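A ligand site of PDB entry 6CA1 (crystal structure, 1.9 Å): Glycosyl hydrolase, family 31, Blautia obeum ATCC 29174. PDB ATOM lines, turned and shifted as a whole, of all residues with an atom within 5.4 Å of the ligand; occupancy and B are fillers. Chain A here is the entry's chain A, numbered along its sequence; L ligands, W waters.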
ATOM      1  N   ASP A  76      21.751 -18.108 -38.673  1.00  0.00           N
ATOM      2  CA  ASP A  76      22.926 -18.112 -37.812  1.00  0.00           C
ATOM      3  C   ASP A  76      24.056 -18.862 -38.517  1.00  0.00           C
ATOM      4  O   ASP A  76      24.183 -20.076 -38.360  1.00  0.00           O
ATOM      5  CB  ASP A  76      22.590 -18.777 -36.472  1.00  0.00           C
ATOM      6  CG  ASP A  76      23.788 -18.867 -35.535  1.00  0.00           C
ATOM      7  OD1 ASP A  76      24.826 -18.229 -35.789  1.00  0.00           O
ATOM      8  OD2 ASP A  76      23.664 -19.585 -34.512  1.00  0.00           O
ATOM      9  N   TRP A 172      33.722 -13.355 -25.554  1.00  0.00           N
ATOM     10  CA  TRP A 172      33.017 -14.546 -25.105  1.00  0.00           C
ATOM     11  C   TRP A 172      33.950 -15.319 -24.176  1.00  0.00           C
ATOM     12  O   TRP A 172      34.862 -16.029 -24.623  1.00  0.00           O
ATOM     13  CB  TRP A 172      32.645 -15.391 -26.326  1.00  0.00           C
ATOM     14  CG  TRP A 172      31.849 -16.619 -26.049  1.00  0.00           C
ATOM     15  CD1 TRP A 172      31.326 -17.029 -24.860  1.00  0.00           C
ATOM     16  CD2 TRP A 172      31.488 -17.619 -27.018  1.00  0.00           C
ATOM     17  NE1 TRP A 172      30.667 -18.237 -25.028  1.00  0.00           N
ATOM     18  CE2 TRP A 172      30.748 -18.613 -26.344  1.00  0.00           C
ATOM     19  CE3 TRP A 172      31.717 -17.764 -28.393  1.00  0.00           C
ATOM     20  CZ2 TRP A 172      30.235 -19.741 -26.997  1.00  0.00           C
ATOM     21  CZ3 TRP A 172      31.211 -18.885 -29.043  1.00  0.00           C
ATOM     22  CH2 TRP A 172      30.480 -19.851 -28.347  1.00  0.00           C
ATOM     23  N   ASP A 200      29.215 -11.053 -21.982  1.00  0.00           N
ATOM     24  CA  ASP A 200      28.672 -12.111 -22.804  1.00  0.00           C
ATOM     25  C   ASP A 200      27.985 -13.124 -21.885  1.00  0.00           C
ATOM     26  O   ASP A 200      27.859 -12.876 -20.678  1.00  0.00           O
ATOM     27  CB  ASP A 200      29.775 -12.758 -23.644  1.00  0.00           C
ATOM     28  CG  ASP A 200      29.265 -13.327 -24.950  1.00  0.00           C
ATOM     29  OD1 ASP A 200      28.156 -13.913 -24.961  1.00  0.00           O
ATOM     30  OD2 ASP A 200      29.968 -13.184 -25.972  1.00  0.00           O
ATOM     31  N   ILE A 201      27.548 -14.243 -22.443  1.00  0.00           N
ATOM     32  CA  ILE A 201      26.539 -15.093 -21.797  1.00  0.00           C
ATOM     33  C   ILE A 201      26.910 -15.666 -20.433  1.00  0.00           C
ATOM     34  O   ILE A 201      26.042 -16.182 -19.720  1.00  0.00           O
ATOM     35  CB  ILE A 201      26.055 -16.239 -22.736  1.00  0.00           C
ATOM     36  CG1 ILE A 201      27.217 -17.098 -23.234  1.00  0.00           C
ATOM     37  CG2 ILE A 201      25.243 -15.668 -23.897  1.00  0.00           C
ATOM     38  CD1 ILE A 201      26.766 -18.299 -24.083  1.00  0.00           C
ATOM     39  N   ILE A 237      24.480  -9.135 -22.541  1.00  0.00           N
ATOM     40  CA  ILE A 237      23.793  -9.821 -23.626  1.00  0.00           C
ATOM     41  C   ILE A 237      22.451 -10.379 -23.138  1.00  0.00           C
ATOM     42  O   ILE A 237      22.323 -10.754 -21.959  1.00  0.00           O
ATOM     43  CB  ILE A 237      24.694 -10.936 -24.169  1.00  0.00           C
ATOM     44  CG1 ILE A 237      24.181 -11.483 -25.510  1.00  0.00           C
ATOM     45  CG2 ILE A 237      24.883 -12.044 -23.125  1.00  0.00           C
ATOM     46  CD1 ILE A 237      25.267 -12.266 -26.275  1.00  0.00           C
ATOM     47  N   ASP A 239      19.559 -13.253 -24.708  1.00  0.00           N
ATOM     48  CA  ASP A 239      19.311 -14.232 -25.778  1.00  0.00           C
ATOM     49  C   ASP A 239      17.826 -14.489 -26.044  1.00  0.00           C
ATOM     50  O   ASP A 239      16.984 -14.188 -25.203  1.00  0.00           O
ATOM     51  CB  ASP A 239      20.027 -15.560 -25.493  1.00  0.00           C
ATOM     52  CG  ASP A 239      21.530 -15.491 -25.773  1.00  0.00           C
ATOM     53  OD1 ASP A 239      21.960 -14.553 -26.482  1.00  0.00           O
ATOM     54  OD2 ASP A 239      22.288 -16.375 -25.310  1.00  0.00           O
ATOM     55  N   TRP A 274      22.015 -22.303 -25.601  1.00  0.00           N
ATOM     56  CA  TRP A 274      23.020 -22.304 -24.535  1.00  0.00           C
ATOM     57  C   TRP A 274      22.558 -22.888 -23.195  1.00  0.00           C
ATOM     58  O   TRP A 274      23.310 -23.646 -22.585  1.00  0.00           O
ATOM     59  CB  TRP A 274      23.681 -20.938 -24.381  1.00  0.00           C
ATOM     60  CG  TRP A 274      24.545 -20.668 -25.567  1.00  0.00           C
ATOM     61  CD1 TRP A 274      24.335 -19.742 -26.533  1.00  0.00           C
ATOM     62  CD2 TRP A 274      25.716 -21.408 -25.943  1.00  0.00           C
ATOM     63  NE1 TRP A 274      25.337 -19.838 -27.487  1.00  0.00           N
ATOM     64  CE2 TRP A 274      26.186 -20.847 -27.152  1.00  0.00           C
ATOM     65  CE3 TRP A 274      26.416 -22.471 -25.381  1.00  0.00           C
ATOM     66  CZ2 TRP A 274      27.329 -21.319 -27.790  1.00  0.00           C
ATOM     67  CZ3 TRP A 274      27.554 -22.932 -26.027  1.00  0.00           C
ATOM     68  CH2 TRP A 274      27.995 -22.362 -27.213  1.00  0.00           C
ATOM     69  N   TRP A 308      22.723  -5.854 -25.724  1.00  0.00           N
ATOM     70  CA  TRP A 308      22.760  -6.440 -27.060  1.00  0.00           C
ATOM     71  C   TRP A 308      21.974  -7.749 -27.137  1.00  0.00           C
ATOM     72  O   TRP A 308      22.046  -8.593 -26.247  1.00  0.00           O
ATOM     73  CB  TRP A 308      24.191  -6.594 -27.606  1.00  0.00           C
ATOM     74  CG  TRP A 308      25.197  -7.299 -26.731  1.00  0.00           C
ATOM     75  CD1 TRP A 308      25.480  -7.046 -25.405  1.00  0.00           C
ATOM     76  CD2 TRP A 308      26.103  -8.329 -27.143  1.00  0.00           C
ATOM     77  NE1 TRP A 308      26.495  -7.872 -24.975  1.00  0.00           N
ATOM     78  CE2 TRP A 308      26.890  -8.675 -26.025  1.00  0.00           C
ATOM     79  CE3 TRP A 308      26.326  -9.000 -28.348  1.00  0.00           C
ATOM     80  CZ2 TRP A 308      27.873  -9.673 -26.074  1.00  0.00           C
ATOM     81  CZ3 TRP A 308      27.303  -9.987 -28.405  1.00  0.00           C
ATOM     82  CH2 TRP A 308      28.065 -10.304 -27.277  1.00  0.00           C
ATOM     83  N   ASP A 310      21.058 -11.306 -28.904  1.00  0.00           N
ATOM     84  CA  ASP A 310      21.771 -12.314 -29.688  1.00  0.00           C
ATOM     85  C   ASP A 310      20.894 -13.535 -29.942  1.00  0.00           C
ATOM     86  O   ASP A 310      19.852 -13.701 -29.299  1.00  0.00           O
ATOM     87  CB  ASP A 310      23.023 -12.752 -28.926  1.00  0.00           C
ATOM     88  CG  ASP A 310      23.954 -13.610 -29.754  1.00  0.00           C
ATOM     89  OD1 ASP A 310      23.846 -13.600 -30.997  1.00  0.00           O
ATOM     90  OD2 ASP A 310      24.790 -14.310 -29.137  1.00  0.00           O
ATOM     91  N   MET A 311      21.319 -14.368 -30.905  1.00  0.00           N
ATOM     92  CA  MET A 311      20.669 -15.661 -31.170  1.00  0.00           C
ATOM     93  C   MET A 311      19.205 -15.499 -31.571  1.00  0.00           C
ATOM     94  O   MET A 311      18.411 -16.420 -31.432  1.00  0.00           O
ATOM     95  CB  MET A 311      20.766 -16.572 -29.927  1.00  0.00           C
ATOM     96  CG  MET A 311      22.192 -16.875 -29.487  1.00  0.00           C
ATOM     97  SD  MET A 311      23.122 -17.739 -30.759  1.00  0.00           S
ATOM     98  CE  MET A 311      22.873 -19.437 -30.259  1.00  0.00           C
ATOM     99  N   PHE A 317      20.122 -25.031 -31.810  1.00  0.00           N
ATOM    100  CA  PHE A 317      21.144 -26.081 -31.931  1.00  0.00           C
ATOM    101  C   PHE A 317      20.470 -27.379 -32.329  1.00  0.00           C
ATOM    102  O   PHE A 317      20.972 -28.123 -33.187  1.00  0.00           O
ATOM    103  CB  PHE A 317      21.937 -26.263 -30.629  1.00  0.00           C
ATOM    104  CG  PHE A 317      22.710 -25.033 -30.218  1.00  0.00           C
ATOM    105  CD1 PHE A 317      22.942 -24.013 -31.124  1.00  0.00           C
ATOM    106  CD2 PHE A 317      23.196 -24.894 -28.921  1.00  0.00           C
ATOM    107  CE1 PHE A 317      23.650 -22.881 -30.757  1.00  0.00           C
ATOM    108  CE2 PHE A 317      23.904 -23.753 -28.539  1.00  0.00           C
ATOM    109  CZ  PHE A 317      24.127 -22.748 -29.463  1.00  0.00           C
ATOM    110  N   ARG A 407      21.499  -8.894 -33.416  1.00  0.00           N
ATOM    111  CA  ARG A 407      22.180  -9.633 -34.485  1.00  0.00           C
ATOM    112  C   ARG A 407      21.262  -9.796 -35.694  1.00  0.00           C
ATOM    113  O   ARG A 407      21.623  -9.424 -36.824  1.00  0.00           O
ATOM    114  CB  ARG A 407      22.657 -10.995 -33.982  1.00  0.00           C
ATOM    115  CG  ARG A 407      23.603 -11.700 -34.985  1.00  0.00           C
ATOM    116  CD  ARG A 407      24.310 -12.883 -34.374  1.00  0.00           C
ATOM    117  NE  ARG A 407      23.420 -14.034 -34.246  1.00  0.00           N
ATOM    118  CZ  ARG A 407      23.826 -15.255 -33.909  1.00  0.00           C
ATOM    119  NH1 ARG A 407      22.949 -16.241 -33.834  1.00  0.00           N
ATOM    120  NH2 ARG A 407      25.110 -15.472 -33.651  1.00  0.00           N
ATOM    121  N   TRP A 420      24.975  -5.307 -35.011  1.00  0.00           N
ATOM    122  CA  TRP A 420      26.374  -5.554 -35.316  1.00  0.00           C
ATOM    123  C   TRP A 420      26.408  -6.622 -36.401  1.00  0.00           C
ATOM    124  O   TRP A 420      25.427  -7.335 -36.603  1.00  0.00           O
ATOM    125  CB  TRP A 420      27.178  -5.904 -34.058  1.00  0.00           C
ATOM    126  CG  TRP A 420      27.252  -7.349 -33.673  1.00  0.00           C
ATOM    127  CD1 TRP A 420      28.278  -8.213 -33.935  1.00  0.00           C
ATOM    128  CD2 TRP A 420      26.287  -8.088 -32.915  1.00  0.00           C
ATOM    129  NE1 TRP A 420      28.000  -9.439 -33.403  1.00  0.00           N
ATOM    130  CE2 TRP A 420      26.789  -9.395 -32.766  1.00  0.00           C
ATOM    131  CE3 TRP A 420      25.050  -7.771 -32.344  1.00  0.00           C
ATOM    132  CZ2 TRP A 420      26.083 -10.391 -32.079  1.00  0.00           C
ATOM    133  CZ3 TRP A 420      24.352  -8.760 -31.654  1.00  0.00           C
ATOM    134  CH2 TRP A 420      24.878 -10.052 -31.530  1.00  0.00           C
ATOM    135  N   GLY A 422      27.543  -9.424 -36.813  1.00  0.00           N
ATOM    136  CA  GLY A 422      27.536 -10.831 -36.429  1.00  0.00           C
ATOM    137  C   GLY A 422      28.919 -11.447 -36.363  1.00  0.00           C
ATOM    138  O   GLY A 422      29.909 -10.761 -36.095  1.00  0.00           O
ATOM    139  N   ASP A 423      28.978 -12.755 -36.603  1.00  0.00           N
ATOM    140  CA  ASP A 423      30.229 -13.505 -36.438  1.00  0.00           C
ATOM    141  C   ASP A 423      31.155 -13.463 -37.645  1.00  0.00           C
ATOM    142  O   ASP A 423      31.183 -14.382 -38.488  1.00  0.00           O
ATOM    143  CB  ASP A 423      29.939 -14.944 -36.002  1.00  0.00           C
ATOM    144  CG  ASP A 423      29.198 -15.018 -34.665  1.00  0.00           C
ATOM    145  OD1 ASP A 423      29.331 -14.068 -33.861  1.00  0.00           O
ATOM    146  OD2 ASP A 423      28.478 -16.014 -34.431  1.00  0.00           O
ATOM    147  N   ASP A 452      32.748  -6.892 -35.527  1.00  0.00           N
ATOM    148  CA  ASP A 452      33.686  -7.242 -34.453  1.00  0.00           C
ATOM    149  C   ASP A 452      35.106  -6.948 -34.932  1.00  0.00           C
ATOM    150  O   ASP A 452      35.651  -7.639 -35.798  1.00  0.00           O
ATOM    151  CB  ASP A 452      33.550  -8.712 -34.050  1.00  0.00           C
ATOM    152  CG  ASP A 452      32.208  -9.027 -33.423  1.00  0.00           C
ATOM    153  OD1 ASP A 452      31.472  -8.085 -33.043  1.00  0.00           O
ATOM    154  OD2 ASP A 452      31.883 -10.228 -33.305  1.00  0.00           O
ATOM    155  N   PHE A 456      35.834 -11.797 -35.080  1.00  0.00           N
ATOM    156  CA  PHE A 456      35.265 -12.594 -34.003  1.00  0.00           C
ATOM    157  C   PHE A 456      35.917 -13.985 -33.908  1.00  0.00           C
ATOM    158  O   PHE A 456      36.487 -14.328 -32.880  1.00  0.00           O
ATOM    159  CB  PHE A 456      33.752 -12.697 -34.189  1.00  0.00           C
ATOM    160  CG  PHE A 456      33.053 -13.613 -33.222  1.00  0.00           C
ATOM    161  CD1 PHE A 456      32.804 -13.219 -31.912  1.00  0.00           C
ATOM    162  CD2 PHE A 456      32.597 -14.863 -33.639  1.00  0.00           C
ATOM    163  CE1 PHE A 456      32.136 -14.065 -31.034  1.00  0.00           C
ATOM    164  CE2 PHE A 456      31.930 -15.706 -32.771  1.00  0.00           C
ATOM    165  CZ  PHE A 456      31.696 -15.309 -31.469  1.00  0.00           C
ATOM    166  N   ARG A 479      33.713  -1.734 -31.697  1.00  0.00           N
ATOM    167  CA  ARG A 479      33.813  -2.747 -30.676  1.00  0.00           C
ATOM    168  C   ARG A 479      34.762  -3.881 -31.029  1.00  0.00           C
ATOM    169  O   ARG A 479      34.619  -4.529 -32.070  1.00  0.00           O
ATOM    170  CB  ARG A 479      32.431  -3.330 -30.383  1.00  0.00           C
ATOM    171  CG  ARG A 479      32.456  -4.564 -29.520  1.00  0.00           C
ATOM    172  CD  ARG A 479      31.061  -5.076 -29.265  1.00  0.00           C
ATOM    173  NE  ARG A 479      30.676  -6.101 -30.224  1.00  0.00           N
ATOM    174  CZ  ARG A 479      29.783  -7.049 -29.974  1.00  0.00           C
ATOM    175  NH1 ARG A 479      29.204  -7.112 -28.782  1.00  0.00           N
ATOM    176  NH2 ARG A 479      29.483  -7.940 -30.906  1.00  0.00           N
ATOM    177  N   HIS A 481      35.639  -7.446 -30.177  1.00  0.00           N
ATOM    178  CA  HIS A 481      34.994  -8.626 -29.558  1.00  0.00           C
ATOM    179  C   HIS A 481      35.517  -9.905 -30.193  1.00  0.00           C
ATOM    180  O   HIS A 481      35.737  -9.944 -31.409  1.00  0.00           O
ATOM    181  CB  HIS A 481      33.470  -8.555 -29.719  1.00  0.00           C
ATOM    182  CG  HIS A 481      32.741  -9.719 -29.121  1.00  0.00           C
ATOM    183  ND1 HIS A 481      32.866 -10.073 -27.786  1.00  0.00           N
ATOM    184  CD2 HIS A 481      31.867 -10.598 -29.661  1.00  0.00           C
ATOM    185  CE1 HIS A 481      32.113 -11.116 -27.541  1.00  0.00           C
ATOM    186  NE2 HIS A 481      31.493 -11.459 -28.659  1.00  0.00           N
ATOM    187  N   ALA A 482      35.735 -10.940 -29.377  1.00  0.00           N
ATOM    188  CA  ALA A 482      36.305 -12.209 -29.876  1.00  0.00           C
ATOM    189  C   ALA A 482      35.544 -13.430 -29.357  1.00  0.00           C
ATOM    190  O   ALA A 482      34.904 -13.376 -28.306  1.00  0.00           O
ATOM    191  CB  ALA A 482      37.783 -12.316 -29.517  1.00  0.00           C
HETATM  192  O1  LIG L   1      26.536 -19.561 -30.185  1.00  0.00           O
HETATM  193  O2  LIG L   1      27.287 -15.375 -26.720  1.00  0.00           O
HETATM  194  O3  LIG L   1      27.167 -13.497 -32.367  1.00  0.00           O
HETATM  195  O4  LIG L   1      28.900 -12.232 -30.491  1.00  0.00           O
HETATM  196  O5  LIG L   1      29.981 -13.895 -28.501  1.00  0.00           O
HETATM  197  C1  LIG L   1      27.132 -18.290 -30.083  1.00  0.00           C
HETATM  198  C2  LIG L   1      28.253 -16.003 -27.444  1.00  0.00           C
HETATM  199  C3  LIG L   1      26.412 -17.185 -29.445  1.00  0.00           C
HETATM  200  C4  LIG L   1      26.970 -15.363 -30.960  1.00  0.00           C
HETATM  201  C5  LIG L   1      27.302 -13.890 -31.014  1.00  0.00           C
HETATM  202  C6  LIG L   1      28.623 -13.604 -30.437  1.00  0.00           C
HETATM  203  C7  LIG L   1      28.700 -14.116 -29.038  1.00  0.00           C
HETATM  204  C8  LIG L   1      28.337 -15.603 -28.906  1.00  0.00           C
HETATM  205  N1  LIG L   1      27.068 -15.894 -29.578  1.00  0.00           N
HETATM  206  O   HOH W   1      24.450 -15.986 -27.064  1.00  0.00           O
HETATM  207  O   HOH W   2      27.839 -21.636 -31.613  1.00  0.00           O
HETATM  208  O   HOH W   3      25.660 -18.258 -32.873  1.00  0.00           O
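Water W1 lies within hydrogen-bond range of the side-chain carboxylate (OD2) of Asp 310, the side-chain carboxylate (OD2) of Asp 239 and an oxygen (O2) of the ligand. Water W3 lies within hydrogen-bond range of OD2 of Asp 76 (2.9 Å), NH2 of Arg 407 (2.9 Å), O1 of the ligand (3.1 Å) and SD of Met 311 (3.3 Å).
Residues that only touch the ligand: Trp 420, Phe 456, Trp 308, Ile 201, Met 311, Trp 172 and Ile 237. Hydrophobic or aromatic side chains that line the ligand: Trp 172, Ile 201, Ile 237, Trp 274, Trp 308, Met 311, Trp 420, Phe 456 and His 481. Within 4 Å of the ligand: Trp 172, Asp 200, Ile 201, Ile 237, Trp 274, Trp 308, Asp 310, Met 311, Arg 407, Trp 420, Asp 423, Phe 456 and His 481.
An oxygen (O2) of the ligand sits at hydrogen-bond distance from the side-chain carboxylate (OD1) of Asp 200 (2.4 Å). OD1 of Asp 423 sits at hydrogen-bond distance from O3 of the ligand. The side-chain carboxylate (OD2) of Asp 310 is in salt-bridge range of a nitrogen (N1) of the ligand (2.8 Å). O5 of the ligand is in hydrogen-bond range of NE2 of His 481 (2.9 Å). The indole nitrogen (NE1) of Trp 274 sits at hydrogen-bond distance from an oxygen (O1) of the ligand. An oxygen (O3) of the ligand lies within hydrogen-bond range of the guanidinium group of Arg 407, at 3.1 Å.
The side-chain carboxylate (OD2) of Asp 423 is in salt-bridge range of the guanidinium group (NH2) of Arg 407 (3.5 Å). The side-chain carboxylate (OD1) of Asp 310 is in salt-bridge range of the guanidinium group (NE) of Arg 407, 3.3 Å away. The side-chain sulfur of Met 311 lies within hydrogen-bond range of the guanidinium group of Arg 407. The guanidinium group (NH1) of Arg 407 lies within salt-bridge range of the side-chain carboxylate (OD1) of Asp 76, 3.4 Å away. N of Trp 172 is in hydrogen-bond range of O of Ala 482, 3.0 Å away.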
